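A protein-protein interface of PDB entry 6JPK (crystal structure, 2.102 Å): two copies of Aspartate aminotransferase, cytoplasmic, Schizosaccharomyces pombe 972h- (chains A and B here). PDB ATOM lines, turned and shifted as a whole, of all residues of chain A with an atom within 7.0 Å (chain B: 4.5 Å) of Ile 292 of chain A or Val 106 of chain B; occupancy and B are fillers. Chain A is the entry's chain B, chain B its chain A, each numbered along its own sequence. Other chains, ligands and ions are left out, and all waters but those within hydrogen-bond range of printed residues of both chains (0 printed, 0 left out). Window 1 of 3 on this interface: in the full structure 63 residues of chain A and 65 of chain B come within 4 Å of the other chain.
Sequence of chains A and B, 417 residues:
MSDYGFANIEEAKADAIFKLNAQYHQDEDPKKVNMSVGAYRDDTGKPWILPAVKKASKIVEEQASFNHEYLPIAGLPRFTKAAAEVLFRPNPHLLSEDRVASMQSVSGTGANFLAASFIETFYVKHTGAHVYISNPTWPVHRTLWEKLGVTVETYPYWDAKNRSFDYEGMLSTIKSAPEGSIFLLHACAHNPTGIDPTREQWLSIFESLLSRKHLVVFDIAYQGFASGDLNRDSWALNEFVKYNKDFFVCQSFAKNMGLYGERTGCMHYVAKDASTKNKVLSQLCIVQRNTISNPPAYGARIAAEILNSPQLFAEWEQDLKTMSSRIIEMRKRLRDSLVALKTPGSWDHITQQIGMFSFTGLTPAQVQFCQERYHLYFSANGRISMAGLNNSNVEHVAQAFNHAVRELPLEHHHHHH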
ATOM      1  N   ILE A  73       0.141  19.241 -35.779  1.00  0.00           N
ATOM      2  CA  ILE A  73       0.859  19.488 -34.522  1.00  0.00           C
ATOM      3  C   ILE A  73       0.643  20.919 -34.031  1.00  0.00           C
ATOM      4  O   ILE A  73       0.442  21.163 -32.832  1.00  0.00           O
ATOM      5  CB  ILE A  73       2.364  19.184 -34.684  1.00  0.00           C
ATOM      6  CG1 ILE A  73       2.605  17.701 -34.937  1.00  0.00           C
ATOM      7  CG2 ILE A  73       3.107  19.560 -33.423  1.00  0.00           C
ATOM      8  CD1 ILE A  73       4.053  17.389 -35.274  1.00  0.00           C
ATOM      9  N   GLN A 104      -1.366  26.505 -31.796  1.00  0.00           N
ATOM     10  CA  GLN A 104      -2.496  26.255 -30.915  1.00  0.00           C
ATOM     11  C   GLN A 104      -2.006  25.513 -29.680  1.00  0.00           C
ATOM     12  O   GLN A 104      -1.198  24.579 -29.762  1.00  0.00           O
ATOM     13  CB  GLN A 104      -3.574  25.455 -31.646  1.00  0.00           C
ATOM     14  CG  GLN A 104      -4.800  25.150 -30.803  1.00  0.00           C
ATOM     15  CD  GLN A 104      -5.764  24.263 -31.549  1.00  0.00           C
ATOM     16  OE1 GLN A 104      -5.821  24.289 -32.783  1.00  0.00           O
ATOM     17  NE2 GLN A 104      -6.518  23.458 -30.811  1.00  0.00           N
ATOM     18  N   SER A 105      -2.468  25.959 -28.524  1.00  0.00           N
ATOM     19  CA  SER A 105      -1.983  25.446 -27.256  1.00  0.00           C
ATOM     20  C   SER A 105      -3.161  25.076 -26.366  1.00  0.00           C
ATOM     21  O   SER A 105      -4.327  25.376 -26.668  1.00  0.00           O
ATOM     22  CB  SER A 105      -1.089  26.469 -26.546  1.00  0.00           C
ATOM     23  OG  SER A 105       0.081  26.732 -27.299  1.00  0.00           O
ATOM     24  N   VAL A 106      -2.836  24.415 -25.253  1.00  0.00           N
ATOM     25  CA  VAL A 106      -3.834  24.061 -24.249  1.00  0.00           C
ATOM     26  C   VAL A 106      -4.086  25.304 -23.397  1.00  0.00           C
ATOM     27  O   VAL A 106      -3.606  25.420 -22.258  1.00  0.00           O
ATOM     28  CB  VAL A 106      -3.388  22.848 -23.412  1.00  0.00           C
ATOM     29  CG1 VAL A 106      -4.522  22.370 -22.507  1.00  0.00           C
ATOM     30  CG2 VAL A 106      -2.952  21.730 -24.342  1.00  0.00           C
ATOM     31  N   LEU A 114       4.748  26.479 -23.659  1.00  0.00           N
ATOM     32  CA  LEU A 114       5.434  26.443 -24.948  1.00  0.00           C
ATOM     33  C   LEU A 114       6.449  27.566 -25.071  1.00  0.00           C
ATOM     34  O   LEU A 114       7.603  27.335 -25.440  1.00  0.00           O
ATOM     35  CB  LEU A 114       4.416  26.555 -26.087  1.00  0.00           C
ATOM     36  CG  LEU A 114       4.113  25.310 -26.899  1.00  0.00           C
ATOM     37  CD1 LEU A 114       3.198  25.696 -28.057  1.00  0.00           C
ATOM     38  CD2 LEU A 114       5.422  24.695 -27.398  1.00  0.00           C
ATOM     39  N   VAL A 287       8.701  20.555 -29.407  1.00  0.00           N
ATOM     40  CA  VAL A 287       8.240  20.633 -28.026  1.00  0.00           C
ATOM     41  C   VAL A 287       6.815  20.109 -27.924  1.00  0.00           C
ATOM     42  O   VAL A 287       6.496  19.286 -27.059  1.00  0.00           O
ATOM     43  CB  VAL A 287       8.360  22.073 -27.496  1.00  0.00           C
ATOM     44  CG1 VAL A 287       7.674  22.197 -26.140  1.00  0.00           C
ATOM     45  CG2 VAL A 287       9.829  22.481 -27.398  1.00  0.00           C
ATOM     46  N   GLN A 288       5.944  20.569 -28.828  1.00  0.00           N
ATOM     47  CA  GLN A 288       4.543  20.162 -28.793  1.00  0.00           C
ATOM     48  C   GLN A 288       4.393  18.668 -29.031  1.00  0.00           C
ATOM     49  O   GLN A 288       3.581  18.002 -28.375  1.00  0.00           O
ATOM     50  CB  GLN A 288       3.757  20.939 -29.841  1.00  0.00           C
ATOM     51  CG  GLN A 288       2.275  20.647 -29.831  1.00  0.00           C
ATOM     52  CD  GLN A 288       1.480  21.837 -29.335  1.00  0.00           C
ATOM     53  OE1 GLN A 288       1.658  22.288 -28.196  1.00  0.00           O
ATOM     54  NE2 GLN A 288       0.591  22.350 -30.185  1.00  0.00           N
ATOM     55  N   ARG A 289       5.160  18.125 -29.976  1.00  0.00           N
ATOM     56  CA  ARG A 289       5.076  16.697 -30.257  1.00  0.00           C
ATOM     57  C   ARG A 289       5.422  15.870 -29.026  1.00  0.00           C
ATOM     58  O   ARG A 289       4.820  14.815 -28.790  1.00  0.00           O
ATOM     59  CB  ARG A 289       5.996  16.344 -31.424  1.00  0.00           C
ATOM     60  CG  ARG A 289       6.333  14.874 -31.519  1.00  0.00           C
ATOM     61  CD  ARG A 289       6.128  14.364 -32.928  1.00  0.00           C
ATOM     62  NE  ARG A 289       6.902  15.144 -33.886  1.00  0.00           N
ATOM     63  CZ  ARG A 289       6.668  15.168 -35.193  1.00  0.00           C
ATOM     64  NH1 ARG A 289       7.426  15.915 -35.987  1.00  0.00           N
ATOM     65  NH2 ARG A 289       5.667  14.457 -35.704  1.00  0.00           N
ATOM     66  N   ASN A 290       6.358  16.347 -28.204  1.00  0.00           N
ATOM     67  CA  ASN A 290       6.849  15.576 -27.070  1.00  0.00           C
ATOM     68  C   ASN A 290       6.167  15.926 -25.752  1.00  0.00           C
ATOM     69  O   ASN A 290       6.666  15.549 -24.686  1.00  0.00           O
ATOM     70  CB  ASN A 290       8.361  15.738 -26.966  1.00  0.00           C
ATOM     71  CG  ASN A 290       9.059  15.006 -28.063  1.00  0.00           C
ATOM     72  OD1 ASN A 290       9.174  13.780 -28.007  1.00  0.00           O
ATOM     73  ND2 ASN A 290       9.457  15.727 -29.115  1.00  0.00           N
ATOM     74  N   THR A 291       5.029  16.616 -25.797  1.00  0.00           N
ATOM     75  CA  THR A 291       4.283  16.909 -24.580  1.00  0.00           C
ATOM     76  C   THR A 291       2.825  16.501 -24.732  1.00  0.00           C
ATOM     77  O   THR A 291       2.313  15.750 -23.901  1.00  0.00           O
ATOM     78  CB  THR A 291       4.367  18.395 -24.220  1.00  0.00           C
ATOM     79  OG1 THR A 291       4.070  19.167 -25.389  1.00  0.00           O
ATOM     80  CG2 THR A 291       5.777  18.753 -23.702  1.00  0.00           C
ATOM     81  N   ILE A 292       2.151  16.997 -25.773  1.00  0.00           N
ATOM     82  CA  ILE A 292       0.736  16.708 -25.994  1.00  0.00           C
ATOM     83  C   ILE A 292       0.454  16.051 -27.337  1.00  0.00           C
ATOM     84  O   ILE A 292      -0.687  15.607 -27.557  1.00  0.00           O
ATOM     85  CB  ILE A 292      -0.134  17.978 -25.850  1.00  0.00           C
ATOM     86  CG1 ILE A 292       0.174  18.981 -26.963  1.00  0.00           C
ATOM     87  CG2 ILE A 292       0.104  18.639 -24.509  1.00  0.00           C
ATOM     88  CD1 ILE A 292      -0.816  20.142 -27.017  1.00  0.00           C
ATOM     89  N   SER A 293       1.427  16.012 -28.250  1.00  0.00           N
ATOM     90  CA  SER A 293       1.302  15.489 -29.614  1.00  0.00           C
ATOM     91  C   SER A 293       0.536  16.447 -30.530  1.00  0.00           C
ATOM     92  O   SER A 293       1.056  16.852 -31.576  1.00  0.00           O
ATOM     93  CB  SER A 293       0.658  14.093 -29.605  1.00  0.00           C
ATOM     94  OG  SER A 293       0.717  13.480 -30.872  1.00  0.00           O
ATOM     95  N   ASN A 294      -0.686  16.822 -30.162  1.00  0.00           N
ATOM     96  CA  ASN A 294      -1.470  17.790 -30.924  1.00  0.00           C
ATOM     97  C   ASN A 294      -2.574  18.330 -30.020  1.00  0.00           C
ATOM     98  O   ASN A 294      -2.913  17.694 -29.014  1.00  0.00           O
ATOM     99  CB  ASN A 294      -2.044  17.162 -32.209  1.00  0.00           C
ATOM    100  CG  ASN A 294      -2.583  15.766 -31.990  1.00  0.00           C
ATOM    101  OD1 ASN A 294      -3.692  15.595 -31.470  1.00  0.00           O
ATOM    102  ND2 ASN A 294      -1.806  14.750 -32.392  1.00  0.00           N
ATOM    103  N   PRO A 295      -3.112  19.518 -30.317  1.00  0.00           N
ATOM    104  CA  PRO A 295      -3.965  20.218 -29.347  1.00  0.00           C
ATOM    105  C   PRO A 295      -5.437  19.880 -29.537  1.00  0.00           C
ATOM    106  O   PRO A 295      -5.826  19.331 -30.578  1.00  0.00           O
ATOM    107  CB  PRO A 295      -3.685  21.695 -29.655  1.00  0.00           C
ATOM    108  CG  PRO A 295      -3.464  21.708 -31.128  1.00  0.00           C
ATOM    109  CD  PRO A 295      -2.764  20.395 -31.456  1.00  0.00           C
ATOM    110  N   PRO A 296      -6.292  20.188 -28.548  1.00  0.00           N
ATOM    111  CA  PRO A 296      -7.705  19.763 -28.616  1.00  0.00           C
ATOM    112  C   PRO A 296      -8.548  20.598 -29.568  1.00  0.00           C
ATOM    113  O   PRO A 296      -8.513  21.832 -29.549  1.00  0.00           O
ATOM    114  CB  PRO A 296      -8.196  19.919 -27.170  1.00  0.00           C
ATOM    115  CG  PRO A 296      -7.268  20.893 -26.551  1.00  0.00           C
ATOM    116  CD  PRO A 296      -5.937  20.717 -27.221  1.00  0.00           C
ATOM    117  N   SER B 105      -5.610  13.370 -18.892  1.00  0.00           N
ATOM    118  CA  SER B 105      -4.455  13.876 -19.615  1.00  0.00           C
ATOM    119  C   SER B 105      -4.862  14.281 -21.026  1.00  0.00           C
ATOM    120  O   SER B 105      -5.958  13.962 -21.504  1.00  0.00           O
ATOM    121  CB  SER B 105      -3.342  12.820 -19.675  1.00  0.00           C
ATOM    122  OG  SER B 105      -3.824  11.625 -20.272  1.00  0.00           O
ATOM    123  N   VAL B 106      -3.951  14.977 -21.700  1.00  0.00           N
ATOM    124  CA  VAL B 106      -4.145  15.331 -23.099  1.00  0.00           C
ATOM    125  C   VAL B 106      -3.849  14.069 -23.901  1.00  0.00           C
ATOM    126  O   VAL B 106      -2.766  13.925 -24.486  1.00  0.00           O
ATOM    127  CB  VAL B 106      -3.239  16.502 -23.520  1.00  0.00           C
ATOM    128  CG1 VAL B 106      -3.534  16.927 -24.957  1.00  0.00           C
ATOM    129  CG2 VAL B 106      -3.423  17.685 -22.570  1.00  0.00           C
ATOM    130  N   SER B 107      -4.805  13.139 -23.885  1.00  0.00           N
ATOM    131  CA  SER B 107      -4.745  11.844 -24.557  1.00  0.00           C
ATOM    132  C   SER B 107      -3.571  10.996 -24.081  1.00  0.00           C
ATOM    133  O   SER B 107      -2.998  11.252 -23.011  1.00  0.00           O
ATOM    134  CB  SER B 107      -4.692  12.026 -26.076  1.00  0.00           C
ATOM    135  OG  SER B 107      -5.380  10.970 -26.745  1.00  0.00           O
ATOM    136  N   GLY B 108      -3.224   9.968 -24.860  1.00  0.00           N
ATOM    137  CA  GLY B 108      -2.175   9.050 -24.437  1.00  0.00           C
ATOM    138  C   GLY B 108      -0.805   9.703 -24.357  1.00  0.00           C
ATOM    139  O   GLY B 108      -0.008   9.387 -23.468  1.00  0.00           O
ATOM    140  N   THR B 109      -0.503  10.614 -25.282  1.00  0.00           N
ATOM    141  CA  THR B 109       0.815  11.249 -25.258  1.00  0.00           C
ATOM    142  C   THR B 109       0.999  12.070 -23.987  1.00  0.00           C
ATOM    143  O   THR B 109       2.045  11.994 -23.332  1.00  0.00           O
ATOM    144  CB  THR B 109       1.012  12.121 -26.494  1.00  0.00           C
ATOM    145  OG1 THR B 109       0.874  11.303 -27.657  1.00  0.00           O
ATOM    146  CG2 THR B 109       2.416  12.745 -26.486  1.00  0.00           C
ATOM    147  N   GLY B 110      -0.020  12.859 -23.624  1.00  0.00           N
ATOM    148  CA  GLY B 110       0.037  13.616 -22.386  1.00  0.00           C
ATOM    149  C   GLY B 110       0.096  12.736 -21.153  1.00  0.00           C
ATOM    150  O   GLY B 110       0.749  13.092 -20.168  1.00  0.00           O
ATOM    151  N   ARG B 263      -8.421  14.788 -27.667  1.00  0.00           N
ATOM    152  CA  ARG B 263      -7.339  14.571 -26.704  1.00  0.00           C
ATOM    153  C   ARG B 263      -7.861  14.057 -25.355  1.00  0.00           C
ATOM    154  O   ARG B 263      -7.705  14.697 -24.310  1.00  0.00           O
ATOM    155  CB  ARG B 263      -6.508  15.847 -26.513  1.00  0.00           C
ATOM    156  CG  ARG B 263      -6.149  16.596 -27.794  1.00  0.00           C
ATOM    157  CD  ARG B 263      -5.472  15.701 -28.819  1.00  0.00           C
ATOM    158  NE  ARG B 263      -4.159  15.205 -28.389  1.00  0.00           N
ATOM    159  CZ  ARG B 263      -3.742  13.958 -28.602  1.00  0.00           C
ATOM    160  NH1 ARG B 263      -2.542  13.580 -28.205  1.00  0.00           N
ATOM    161  NH2 ARG B 263      -4.549  13.072 -29.187  1.00  0.00           N
ATOM    162  N   ILE B 292      -0.452  22.492 -18.265  1.00  0.00           N
ATOM    163  CA  ILE B 292      -1.702  22.716 -18.989  1.00  0.00           C
ATOM    164  C   ILE B 292      -2.745  23.353 -18.083  1.00  0.00           C
ATOM    165  O   ILE B 292      -3.793  23.800 -18.562  1.00  0.00           O
ATOM    166  CB  ILE B 292      -2.247  21.404 -19.581  1.00  0.00           C
ATOM    167  CG1 ILE B 292      -2.660  20.438 -18.465  1.00  0.00           C
ATOM    168  CG2 ILE B 292      -1.224  20.772 -20.557  1.00  0.00           C
ATOM    169  CD1 ILE B 292      -3.523  19.273 -18.952  1.00  0.00           C
ATOM    170  N   PRO B 296      -8.763  19.175 -21.183  1.00  0.00           N
ATOM    171  CA  PRO B 296      -9.951  19.534 -21.987  1.00  0.00           C
ATOM    172  C   PRO B 296     -11.175  18.684 -21.660  1.00  0.00           C
ATOM    173  O   PRO B 296     -11.107  17.456 -21.615  1.00  0.00           O
ATOM    174  CB  PRO B 296      -9.488  19.297 -23.433  1.00  0.00           C
ATOM    175  CG  PRO B 296      -8.395  18.289 -23.320  1.00  0.00           C
ATOM    176  CD  PRO B 296      -7.689  18.595 -22.010  1.00  0.00           C
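The backbone carbonyl oxygen of Asn 294 of chain A is in hydrogen-bond range of the guanidinium group of Arg 263 of chain B (2.9 Å).
The guanidinium group of Arg 263 of chain B sits at hydrogen-bond distance from the backbone carbonyl oxygen of Ile 292 of chain A.
N of Ser 107 of chain B is in hydrogen-bond range of O of Arg 263 of chain B, 3.3 Å away.
The backbone carbonyl oxygen of Gln 288 of chain A sits at hydrogen-bond distance from the backbone NH of Ser 293 of chain A, 2.9 Å away.
O of Val 287 of chain A sits at hydrogen-bond distance from OG1 of Thr 291 of chain A (2.9 Å).
OG of Ser 293 of chain A lies within hydrogen-bond range of ND2 of Asn 294 of chain A (3.2 Å).
NE2 of Gln 104 of chain A lies within hydrogen-bond range of O of Pro 296 of chain A (2.9 Å).
The side-chain hydroxyl (OG1) of Thr 291 of chain A sits at hydrogen-bond distance from the backbone carbonyl oxygen (O) of Gln 288 of chain A.
Among the printed residues, pairs that only touch across the chains: Ser 293 of chain A with Thr 109 of chain B, Thr 291 of chain A with Gly 110 of chain B, Ser 293 of chain A with Arg 263 of chain B, Pro 296 of chain A with Arg 263 of chain B, Ile 292 of chain A with Val 106 of chain B, Pro 295 of chain A with Arg 263 of chain B, Thr 291 of chain A with Thr 109 of chain B, Val 106 of chain A with Ile 292 of chain B, Arg 289 of chain A with Thr 109 of chain B and Ile 292 of chain A with Thr 109 of chain B.
Ile 292 of chain A touches three residues of chain B.
Val 106 of chain B touches just one residue of chain A: Ile 292 (3.7 Å).
Of the printed residues of chain A, Thr 109 of chain B touches Arg 289, Thr 291, Ile 292 and Ser 293.
Of the printed residues of chain A, Ile 292 of chain B touches Val 106.
Printed residues of chain B within 4 Å of Pro 296 of chain A: Arg 263.
Printed residues of chain A within 4 Å of Arg 263 of chain B: Ile 292 (2.8 Å), Ser 293 (3.5 Å), Asn 294 (2.9 Å), Pro 295 (3.8 Å) and Pro 296 (3.6 Å).
Of the printed residues of chain B, Val 106 of chain A touches Ile 292 (3.8 Å).
Ser 107 of chain B touches none of the printed residues of chain A.
The nearest printed residue of chain B that does not touch Ile 292 of chain A is Gly 110 of chain B (4.6 Å).
The nearest residue of chain A that does not touch Val 106 of chain B is Asn 294 of chain A (4.2 Å).
The nearest printed residue of chain B that does not touch Asn 294 of chain A is Val 106 of chain B (4.2 Å).
Of the 15 printed residues of chain A, 8 touch a printed residue of chain B.
Hydrophobic or aromatic side chains of chain A within 4 Å of the printed part of chain B: Val 106, Ile 292 and Pro 296.
Hydrophobic or aromatic side chains of chain B that line the printed part of chain A: Val 106 and Ile 292.
Among the printed residues, no Asp or Glu carboxylate lies within 4 Å of a Lys or Arg side-chain nitrogen of the other chain.
Val 106 of chain A touches Ile 292 of chain B, and with the chains exchanged Ile 292 of chain A touches Val 106 of chain B.
Positions printed for both chains: 105, 106, 292 and 296.
Of the 12 pairs that touch across the chains among the printed residues, 2 have their exchanged pair printed and touching as well.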
